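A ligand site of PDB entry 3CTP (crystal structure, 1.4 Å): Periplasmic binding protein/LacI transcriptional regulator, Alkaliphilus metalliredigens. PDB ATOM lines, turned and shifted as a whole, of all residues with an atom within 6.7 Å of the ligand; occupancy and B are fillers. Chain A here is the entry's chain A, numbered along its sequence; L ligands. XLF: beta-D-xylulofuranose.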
ATOM      1  N   ASN A  72      23.497  24.199 -14.079  1.00  0.00           N
ATOM      2  CA  ASN A  72      22.200  23.959 -14.735  1.00  0.00           C
ATOM      3  C   ASN A  72      22.384  24.110 -16.253  1.00  0.00           C
ATOM      4  O   ASN A  72      22.802  25.175 -16.718  1.00  0.00           O
ATOM      5  CB  ASN A  72      21.198  24.990 -14.199  1.00  0.00           C
ATOM      6  CG  ASN A  72      19.828  24.862 -14.833  1.00  0.00           C
ATOM      7  OD1 ASN A  72      19.660  24.240 -15.896  1.00  0.00           O
ATOM      8  ND2 ASN A  72      18.824  25.447 -14.154  1.00  0.00           N
ATOM      9  N   PRO A  73      22.140  23.024 -16.997  1.00  0.00           N
ATOM     10  CA  PRO A  73      22.331  23.051 -18.447  1.00  0.00           C
ATOM     11  C   PRO A  73      21.730  24.258 -19.107  1.00  0.00           C
ATOM     12  O   PRO A  73      22.303  24.804 -20.038  1.00  0.00           O
ATOM     13  CB  PRO A  73      21.606  21.777 -18.900  1.00  0.00           C
ATOM     14  CG  PRO A  73      21.931  20.811 -17.802  1.00  0.00           C
ATOM     15  CD  PRO A  73      21.736  21.676 -16.527  1.00  0.00           C
ATOM     16  N   PHE A  74      20.571  24.709 -18.633  1.00  0.00           N
ATOM     17  CA  PHE A  74      19.935  25.846 -19.313  1.00  0.00           C
ATOM     18  C   PHE A  74      20.866  27.077 -19.235  1.00  0.00           C
ATOM     19  O   PHE A  74      21.024  27.819 -20.208  1.00  0.00           O
ATOM     20  CB  PHE A  74      18.589  26.201 -18.634  1.00  0.00           C
ATOM     21  CG  PHE A  74      17.964  27.449 -19.205  1.00  0.00           C
ATOM     22  CD1 PHE A  74      17.290  27.390 -20.409  1.00  0.00           C
ATOM     23  CD2 PHE A  74      18.113  28.670 -18.563  1.00  0.00           C
ATOM     24  CE1 PHE A  74      16.727  28.554 -20.973  1.00  0.00           C
ATOM     25  CE2 PHE A  74      17.586  29.841 -19.108  1.00  0.00           C
ATOM     26  CZ  PHE A  74      16.896  29.777 -20.316  1.00  0.00           C
ATOM     27  N   PHE A  75      21.478  27.294 -18.083  1.00  0.00           N
ATOM     28  CA  PHE A  75      22.322  28.493 -17.983  1.00  0.00           C
ATOM     29  C   PHE A  75      23.641  28.341 -18.726  1.00  0.00           C
ATOM     30  O   PHE A  75      24.190  29.358 -19.195  1.00  0.00           O
ATOM     31  CB  PHE A  75      22.568  28.900 -16.530  1.00  0.00           C
ATOM     32  CG  PHE A  75      21.341  29.497 -15.895  1.00  0.00           C
ATOM     33  CD1 PHE A  75      20.855  30.720 -16.346  1.00  0.00           C
ATOM     34  CD2 PHE A  75      20.671  28.819 -14.913  1.00  0.00           C
ATOM     35  CE1 PHE A  75      19.668  31.267 -15.787  1.00  0.00           C
ATOM     36  CE2 PHE A  75      19.496  29.345 -14.368  1.00  0.00           C
ATOM     37  CZ  PHE A  75      19.004  30.574 -14.790  1.00  0.00           C
ATOM     38  N   ARG A 124      18.277  36.316 -12.689  1.00  0.00           N
ATOM     39  CA  ARG A 124      17.621  35.833 -11.499  1.00  0.00           C
ATOM     40  C   ARG A 124      18.099  36.612 -10.254  1.00  0.00           C
ATOM     41  O   ARG A 124      18.363  36.052  -9.174  1.00  0.00           O
ATOM     42  CB  ARG A 124      17.813  34.308 -11.362  1.00  0.00           C
ATOM     43  CG  ARG A 124      16.653  33.625 -10.672  1.00  0.00           C
ATOM     44  CD  ARG A 124      16.495  32.194 -11.173  1.00  0.00           C
ATOM     45  NE  ARG A 124      17.578  31.331 -10.688  1.00  0.00           N
ATOM     46  CZ  ARG A 124      17.729  30.064 -11.089  1.00  0.00           C
ATOM     47  NH1 ARG A 124      18.702  29.307 -10.600  1.00  0.00           N
ATOM     48  NH2 ARG A 124      16.870  29.554 -11.982  1.00  0.00           N
ATOM     49  N   PHE A 141      17.725  39.311 -16.565  1.00  0.00           N
ATOM     50  CA  PHE A 141      16.976  38.115 -17.000  1.00  0.00           C
ATOM     51  C   PHE A 141      16.049  37.607 -15.865  1.00  0.00           C
ATOM     52  O   PHE A 141      16.523  37.340 -14.750  1.00  0.00           O
ATOM     53  CB  PHE A 141      17.952  37.005 -17.480  1.00  0.00           C
ATOM     54  CG  PHE A 141      17.275  35.701 -17.862  1.00  0.00           C
ATOM     55  CD1 PHE A 141      16.410  35.642 -18.952  1.00  0.00           C
ATOM     56  CD2 PHE A 141      17.513  34.544 -17.135  1.00  0.00           C
ATOM     57  CE1 PHE A 141      15.791  34.420 -19.299  1.00  0.00           C
ATOM     58  CE2 PHE A 141      16.902  33.328 -17.471  1.00  0.00           C
ATOM     59  CZ  PHE A 141      16.048  33.272 -18.542  1.00  0.00           C
ATOM     60  N   GLU A 142      14.730  37.549 -16.155  1.00  0.00           N
ATOM     61  CA  GLU A 142      13.677  37.051 -15.236  1.00  0.00           C
ATOM     62  C   GLU A 142      13.254  37.938 -14.096  1.00  0.00           C
ATOM     63  O   GLU A 142      12.074  38.323 -14.018  1.00  0.00           O
ATOM     64  CB  GLU A 142      14.005  35.655 -14.707  1.00  0.00           C
ATOM     65  CG  GLU A 142      13.929  34.649 -15.843  1.00  0.00           C
ATOM     66  CD  GLU A 142      14.085  33.192 -15.389  1.00  0.00           C
ATOM     67  OE1 GLU A 142      13.816  32.294 -16.227  1.00  0.00           O
ATOM     68  OE2 GLU A 142      14.467  32.962 -14.223  1.00  0.00           O
ATOM     69  N   ASN A 143      14.150  38.179 -13.144  1.00  0.00           N
ATOM     70  CA  ASN A 143      13.728  38.884 -11.952  1.00  0.00           C
ATOM     71  C   ASN A 143      13.871  40.381 -12.169  1.00  0.00           C
ATOM     72  O   ASN A 143      14.902  40.844 -12.659  1.00  0.00           O
ATOM     73  CB  ASN A 143      14.575  38.475 -10.742  1.00  0.00           C
ATOM     74  CG  ASN A 143      14.193  37.138 -10.160  1.00  0.00           C
ATOM     75  OD1 ASN A 143      13.313  36.442 -10.659  1.00  0.00           O
ATOM     76  ND2 ASN A 143      14.871  36.773  -9.070  1.00  0.00           N
ATOM     77  N   SER A 154      11.251  34.503 -20.609  1.00  0.00           N
ATOM     78  CA  SER A 154      10.308  33.733 -21.412  1.00  0.00           C
ATOM     79  C   SER A 154       8.893  33.947 -20.869  1.00  0.00           C
ATOM     80  O   SER A 154       8.729  34.494 -19.791  1.00  0.00           O
ATOM     81  CB  SER A 154      10.616  32.240 -21.385  1.00  0.00           C
ATOM     82  OG  SER A 154      11.889  31.966 -21.995  1.00  0.00           O
ATOM     83  N   ASN A 156       6.651  32.701 -18.972  1.00  0.00           N
ATOM     84  CA  ASN A 156       6.546  31.641 -17.979  1.00  0.00           C
ATOM     85  C   ASN A 156       5.132  31.355 -17.493  1.00  0.00           C
ATOM     86  O   ASN A 156       4.781  30.209 -17.190  1.00  0.00           O
ATOM     87  CB  ASN A 156       7.483  32.008 -16.835  1.00  0.00           C
ATOM     88  CG  ASN A 156       8.930  31.816 -17.231  1.00  0.00           C
ATOM     89  OD1 ASN A 156       9.304  30.729 -17.683  1.00  0.00           O
ATOM     90  ND2 ASN A 156       9.733  32.904 -17.152  1.00  0.00           N
ATOM     91  N   PHE A 184      12.308  32.960  -7.276  1.00  0.00           N
ATOM     92  CA  PHE A 184      12.456  32.970  -8.734  1.00  0.00           C
ATOM     93  C   PHE A 184      11.127  33.428  -9.324  1.00  0.00           C
ATOM     94  O   PHE A 184      10.150  32.664  -9.333  1.00  0.00           O
ATOM     95  CB  PHE A 184      12.733  31.558  -9.279  1.00  0.00           C
ATOM     96  CG  PHE A 184      13.998  30.889  -8.758  1.00  0.00           C
ATOM     97  CD1 PHE A 184      14.989  31.597  -8.074  1.00  0.00           C
ATOM     98  CD2 PHE A 184      14.190  29.527  -9.025  1.00  0.00           C
ATOM     99  CE1 PHE A 184      16.161  30.925  -7.611  1.00  0.00           C
ATOM    100  CE2 PHE A 184      15.346  28.882  -8.615  1.00  0.00           C
ATOM    101  CZ  PHE A 184      16.324  29.590  -7.913  1.00  0.00           C
ATOM    102  N   GLU A 185      11.067  34.672  -9.814  1.00  0.00           N
ATOM    103  CA  GLU A 185       9.829  35.155 -10.396  1.00  0.00           C
ATOM    104  C   GLU A 185       9.328  34.201 -11.492  1.00  0.00           C
ATOM    105  O   GLU A 185       8.124  34.043 -11.677  1.00  0.00           O
ATOM    106  CB  GLU A 185      10.018  36.572 -10.989  1.00  0.00           C
ATOM    107  CG  GLU A 185      10.183  37.630  -9.916  1.00  0.00           C
ATOM    108  CD  GLU A 185      10.200  39.039 -10.481  1.00  0.00           C
ATOM    109  OE1 GLU A 185       9.432  39.323 -11.422  1.00  0.00           O
ATOM    110  OE2 GLU A 185      11.040  39.817 -10.013  1.00  0.00           O
ATOM    111  N   ALA A 186      10.254  33.624 -12.246  1.00  0.00           N
ATOM    112  CA  ALA A 186       9.850  32.774 -13.365  1.00  0.00           C
ATOM    113  C   ALA A 186       9.095  31.550 -12.889  1.00  0.00           C
ATOM    114  O   ALA A 186       8.100  31.155 -13.488  1.00  0.00           O
ATOM    115  CB  ALA A 186      11.067  32.361 -14.188  1.00  0.00           C
ATOM    116  N   THR A 187       9.607  30.902 -11.841  1.00  0.00           N
ATOM    117  CA  THR A 187       8.909  29.689 -11.392  1.00  0.00           C
ATOM    118  C   THR A 187       7.606  30.027 -10.694  1.00  0.00           C
ATOM    119  O   THR A 187       6.661  29.209 -10.693  1.00  0.00           O
ATOM    120  CB  THR A 187       9.822  28.764 -10.541  1.00  0.00           C
ATOM    121  OG1 THR A 187      10.301  29.456  -9.390  1.00  0.00           O
ATOM    122  CG2 THR A 187      11.030  28.352 -11.359  1.00  0.00           C
ATOM    123  N   ARG A 190       5.222  30.215 -13.487  1.00  0.00           N
ATOM    124  CA  ARG A 190       4.852  28.883 -13.959  1.00  0.00           C
ATOM    125  C   ARG A 190       3.834  28.225 -13.036  1.00  0.00           C
ATOM    126  O   ARG A 190       2.874  27.591 -13.469  1.00  0.00           O
ATOM    127  CB  ARG A 190       6.081  27.954 -14.100  1.00  0.00           C
ATOM    128  CG  ARG A 190       7.041  28.456 -15.158  1.00  0.00           C
ATOM    129  CD  ARG A 190       8.391  27.739 -15.116  1.00  0.00           C
ATOM    130  NE  ARG A 190       9.346  28.507 -15.918  1.00  0.00           N
ATOM    131  CZ  ARG A 190      10.660  28.311 -15.923  1.00  0.00           C
ATOM    132  NH1 ARG A 190      11.206  27.338 -15.183  1.00  0.00           N
ATOM    133  NH2 ARG A 190      11.422  29.101 -16.661  1.00  0.00           N
ATOM    134  N   ASP A 213      17.511  25.674  -6.913  1.00  0.00           N
ATOM    135  CA  ASP A 213      17.686  25.070  -8.234  1.00  0.00           C
ATOM    136  C   ASP A 213      18.630  23.877  -8.049  1.00  0.00           C
ATOM    137  O   ASP A 213      19.152  23.621  -6.955  1.00  0.00           O
ATOM    138  CB  ASP A 213      18.311  26.127  -9.180  1.00  0.00           C
ATOM    139  CG  ASP A 213      18.183  25.784 -10.649  1.00  0.00           C
ATOM    140  OD1 ASP A 213      17.613  24.718 -10.997  1.00  0.00           O
ATOM    141  OD2 ASP A 213      18.642  26.625 -11.458  1.00  0.00           O
ATOM    142  N   PHE A 238       9.462  22.146 -12.193  1.00  0.00           N
ATOM    143  CA  PHE A 238       9.714  23.534 -12.592  1.00  0.00           C
ATOM    144  C   PHE A 238      10.822  23.740 -13.614  1.00  0.00           C
ATOM    145  O   PHE A 238      10.846  24.785 -14.283  1.00  0.00           O
ATOM    146  CB  PHE A 238       9.962  24.425 -11.351  1.00  0.00           C
ATOM    147  CG  PHE A 238      11.244  24.105 -10.601  1.00  0.00           C
ATOM    148  CD1 PHE A 238      12.420  24.808 -10.874  1.00  0.00           C
ATOM    149  CD2 PHE A 238      11.258  23.162  -9.579  1.00  0.00           C
ATOM    150  CE1 PHE A 238      13.563  24.518 -10.170  1.00  0.00           C
ATOM    151  CE2 PHE A 238      12.400  22.880  -8.859  1.00  0.00           C
ATOM    152  CZ  PHE A 238      13.561  23.571  -9.153  1.00  0.00           C
ATOM    153  N   ASN A 239      11.782  22.818 -13.717  1.00  0.00           N
ATOM    154  CA  ASN A 239      12.709  22.888 -14.848  1.00  0.00           C
ATOM    155  C   ASN A 239      13.247  21.528 -15.203  1.00  0.00           C
ATOM    156  O   ASN A 239      12.934  20.545 -14.525  1.00  0.00           O
ATOM    157  CB  ASN A 239      13.833  23.929 -14.647  1.00  0.00           C
ATOM    158  CG  ASN A 239      14.820  23.543 -13.585  1.00  0.00           C
ATOM    159  OD1 ASN A 239      14.893  22.392 -13.198  1.00  0.00           O
ATOM    160  ND2 ASN A 239      15.605  24.535 -13.091  1.00  0.00           N
ATOM    161  N   ASP A 240      13.952  21.451 -16.332  1.00  0.00           N
ATOM    162  CA  ASP A 240      14.360  20.153 -16.845  1.00  0.00           C
ATOM    163  C   ASP A 240      15.394  19.454 -15.974  1.00  0.00           C
ATOM    164  O   ASP A 240      15.343  18.242 -15.818  1.00  0.00           O
ATOM    165  CB  ASP A 240      14.913  20.252 -18.281  1.00  0.00           C
ATOM    166  CG  ASP A 240      13.841  20.571 -19.310  1.00  0.00           C
ATOM    167  OD1 ASP A 240      12.630  20.467 -19.006  1.00  0.00           O
ATOM    168  OD2 ASP A 240      14.240  20.906 -20.456  1.00  0.00           O
ATOM    169  N   ILE A 241      16.346  20.215 -15.429  1.00  0.00           N
ATOM    170  CA  ILE A 241      17.377  19.567 -14.596  1.00  0.00           C
ATOM    171  C   ILE A 241      16.760  19.037 -13.289  1.00  0.00           C
ATOM    172  O   ILE A 241      17.095  17.924 -12.847  1.00  0.00           O
ATOM    173  CB  ILE A 241      18.626  20.485 -14.388  1.00  0.00           C
ATOM    174  CG1 ILE A 241      19.728  19.747 -13.627  1.00  0.00           C
ATOM    175  CG2 ILE A 241      18.231  21.785 -13.714  1.00  0.00           C
ATOM    176  CD1 ILE A 241      20.325  18.609 -14.442  1.00  0.00           C
ATOM    177  N   PHE A 266      10.516  21.977 -17.845  1.00  0.00           N
ATOM    178  CA  PHE A 266      10.505  23.297 -18.452  1.00  0.00           C
ATOM    179  C   PHE A 266      11.921  23.668 -18.800  1.00  0.00           C
ATOM    180  O   PHE A 266      12.814  23.479 -17.972  1.00  0.00           O
ATOM    181  CB  PHE A 266       9.956  24.336 -17.449  1.00  0.00           C
ATOM    182  CG  PHE A 266       9.304  25.551 -18.078  1.00  0.00           C
ATOM    183  CD1 PHE A 266       7.915  25.693 -18.065  1.00  0.00           C
ATOM    184  CD2 PHE A 266      10.066  26.582 -18.607  1.00  0.00           C
ATOM    185  CE1 PHE A 266       7.303  26.823 -18.604  1.00  0.00           C
ATOM    186  CE2 PHE A 266       9.471  27.710 -19.156  1.00  0.00           C
ATOM    187  CZ  PHE A 266       8.066  27.817 -19.159  1.00  0.00           C
ATOM    188  N   ASP A 267      12.110  24.218 -20.004  1.00  0.00           N
ATOM    189  CA  ASP A 267      13.343  24.828 -20.511  1.00  0.00           C
ATOM    190  C   ASP A 267      13.655  24.378 -21.942  1.00  0.00           C
ATOM    191  O   ASP A 267      14.113  25.168 -22.757  1.00  0.00           O
ATOM    192  CB  ASP A 267      14.608  24.454 -19.735  1.00  0.00           C
ATOM    193  CG  ASP A 267      14.730  25.147 -18.395  1.00  0.00           C
ATOM    194  OD1 ASP A 267      14.060  26.186 -18.151  1.00  0.00           O
ATOM    195  OD2 ASP A 267      15.567  24.650 -17.594  1.00  0.00           O
ATOM    196  N   SER A 269      16.260  22.349 -22.127  1.00  0.00           N
ATOM    197  CA  SER A 269      17.715  22.286 -22.050  1.00  0.00           C
ATOM    198  C   SER A 269      18.231  20.885 -22.432  1.00  0.00           C
ATOM    199  O   SER A 269      17.455  19.911 -22.579  1.00  0.00           O
ATOM    200  CB  SER A 269      18.205  22.666 -20.653  1.00  0.00           C
ATOM    201  OG  SER A 269      17.835  21.673 -19.710  1.00  0.00           O
ATOM    202  N   GLN A 284      12.085  27.184 -23.776  1.00  0.00           N
ATOM    203  CA  GLN A 284      12.504  28.597 -23.741  1.00  0.00           C
ATOM    204  C   GLN A 284      13.377  28.910 -24.932  1.00  0.00           C
ATOM    205  O   GLN A 284      14.323  28.140 -25.221  1.00  0.00           O
ATOM    206  CB  GLN A 284      13.329  28.895 -22.468  1.00  0.00           C
ATOM    207  CG  GLN A 284      12.553  28.791 -21.191  1.00  0.00           C
ATOM    208  CD  GLN A 284      13.248  29.566 -20.075  1.00  0.00           C
ATOM    209  OE1 GLN A 284      13.304  30.785 -20.123  1.00  0.00           O
ATOM    210  NE2 GLN A 284      13.732  28.854 -19.037  1.00  0.00           N
HETATM  211  O4  XLF L   1      14.352  30.537 -13.022  1.00  0.00           O
HETATM  212  C4  XLF L   1      13.918  29.494 -13.900  1.00  0.00           C
HETATM  213  C5  XLF L   1      14.050  28.183 -13.151  1.00  0.00           C
HETATM  214  O5  XLF L   1      15.157  27.496 -13.745  1.00  0.00           O
HETATM  215  C3  XLF L   1      14.850  29.362 -15.086  1.00  0.00           C
HETATM  216  O3  XLF L   1      14.258  29.835 -16.300  1.00  0.00           O
HETATM  217  C2  XLF L   1      15.076  27.875 -15.121  1.00  0.00           C
HETATM  218  O2  XLF L   1      13.951  27.199 -15.722  1.00  0.00           O
HETATM  219  C1  XLF L   1      16.366  27.485 -15.807  1.00  0.00           C
HETATM  220  O1  XLF L   1      16.559  26.067 -15.679  1.00  0.00           O
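The side-chain amide nitrogen (ND2) of Asn 72 lies within hydrogen-bond range of an oxygen (O1) of the ligand (2.8 Å).
The side-chain amide nitrogen (ND2) of Asn 239 lies within hydrogen-bond range of an oxygen (O5) of the ligand (3.1 Å).
An oxygen (O2) of the ligand sits at hydrogen-bond distance from the guanidinium group (NH1) of Arg 190.
The side-chain carboxylate of Glu 142 is in hydrogen-bond range of an oxygen (O3) of the ligand (2.5 Å).
The side-chain amide nitrogen (NE2) of Gln 284 sits at hydrogen-bond distance from an oxygen (O3) of the ligand (3.0 Å).
The side-chain carboxylate (OD2) of Asp 267 sits at hydrogen-bond distance from an oxygen (O1) of the ligand, 2.6 Å away.
The guanidinium group (NH2) of Arg 124 sits at hydrogen-bond distance from an oxygen (O4) of the ligand (2.9 Å).
The side-chain amide oxygen (OE1) of Gln 284 lies within hydrogen-bond range of the side-chain hydroxyl (OG) of Ser 154 (2.6 Å).
NH1 of Arg 124 lies within salt-bridge range of OD2 of Asp 213.
The side-chain amide nitrogen of Asn 239 is in hydrogen-bond range of the side-chain carboxylate of Asp 213 (2.9 Å).
The side-chain amide nitrogen (ND2) of Asn 72 sits at hydrogen-bond distance from the side-chain carboxylate (OD2) of Asp 213.
The backbone carbonyl oxygen of Phe 141 is in hydrogen-bond range of the backbone NH of Arg 124 (2.9 Å).
OG1 of Thr 187 sits at hydrogen-bond distance from O of Phe 184 (3.2 Å).
OD1 of Asn 156 lies within hydrogen-bond range of NE of Arg 190, at 2.8 Å.
The side-chain amide oxygen of Asn 239 sits close to the backbone NH of Ile 241.
Phe 74 touches the ligand.
CE2 of Phe 75 touches C1 of the ligand, 3.9 Å away.
CB of Ala 186 touches O4 of the ligand, at 3.9 Å.
CG2 of Thr 187 touches C5 of the ligand, at 3.5 Å.
Within 4 Å of the ligand: Asn 72, Phe 74, Phe 75, Arg 124, Glu 142, Ala 186, Thr 187, Arg 190, Asn 239, Asp 267 and Gln 284.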
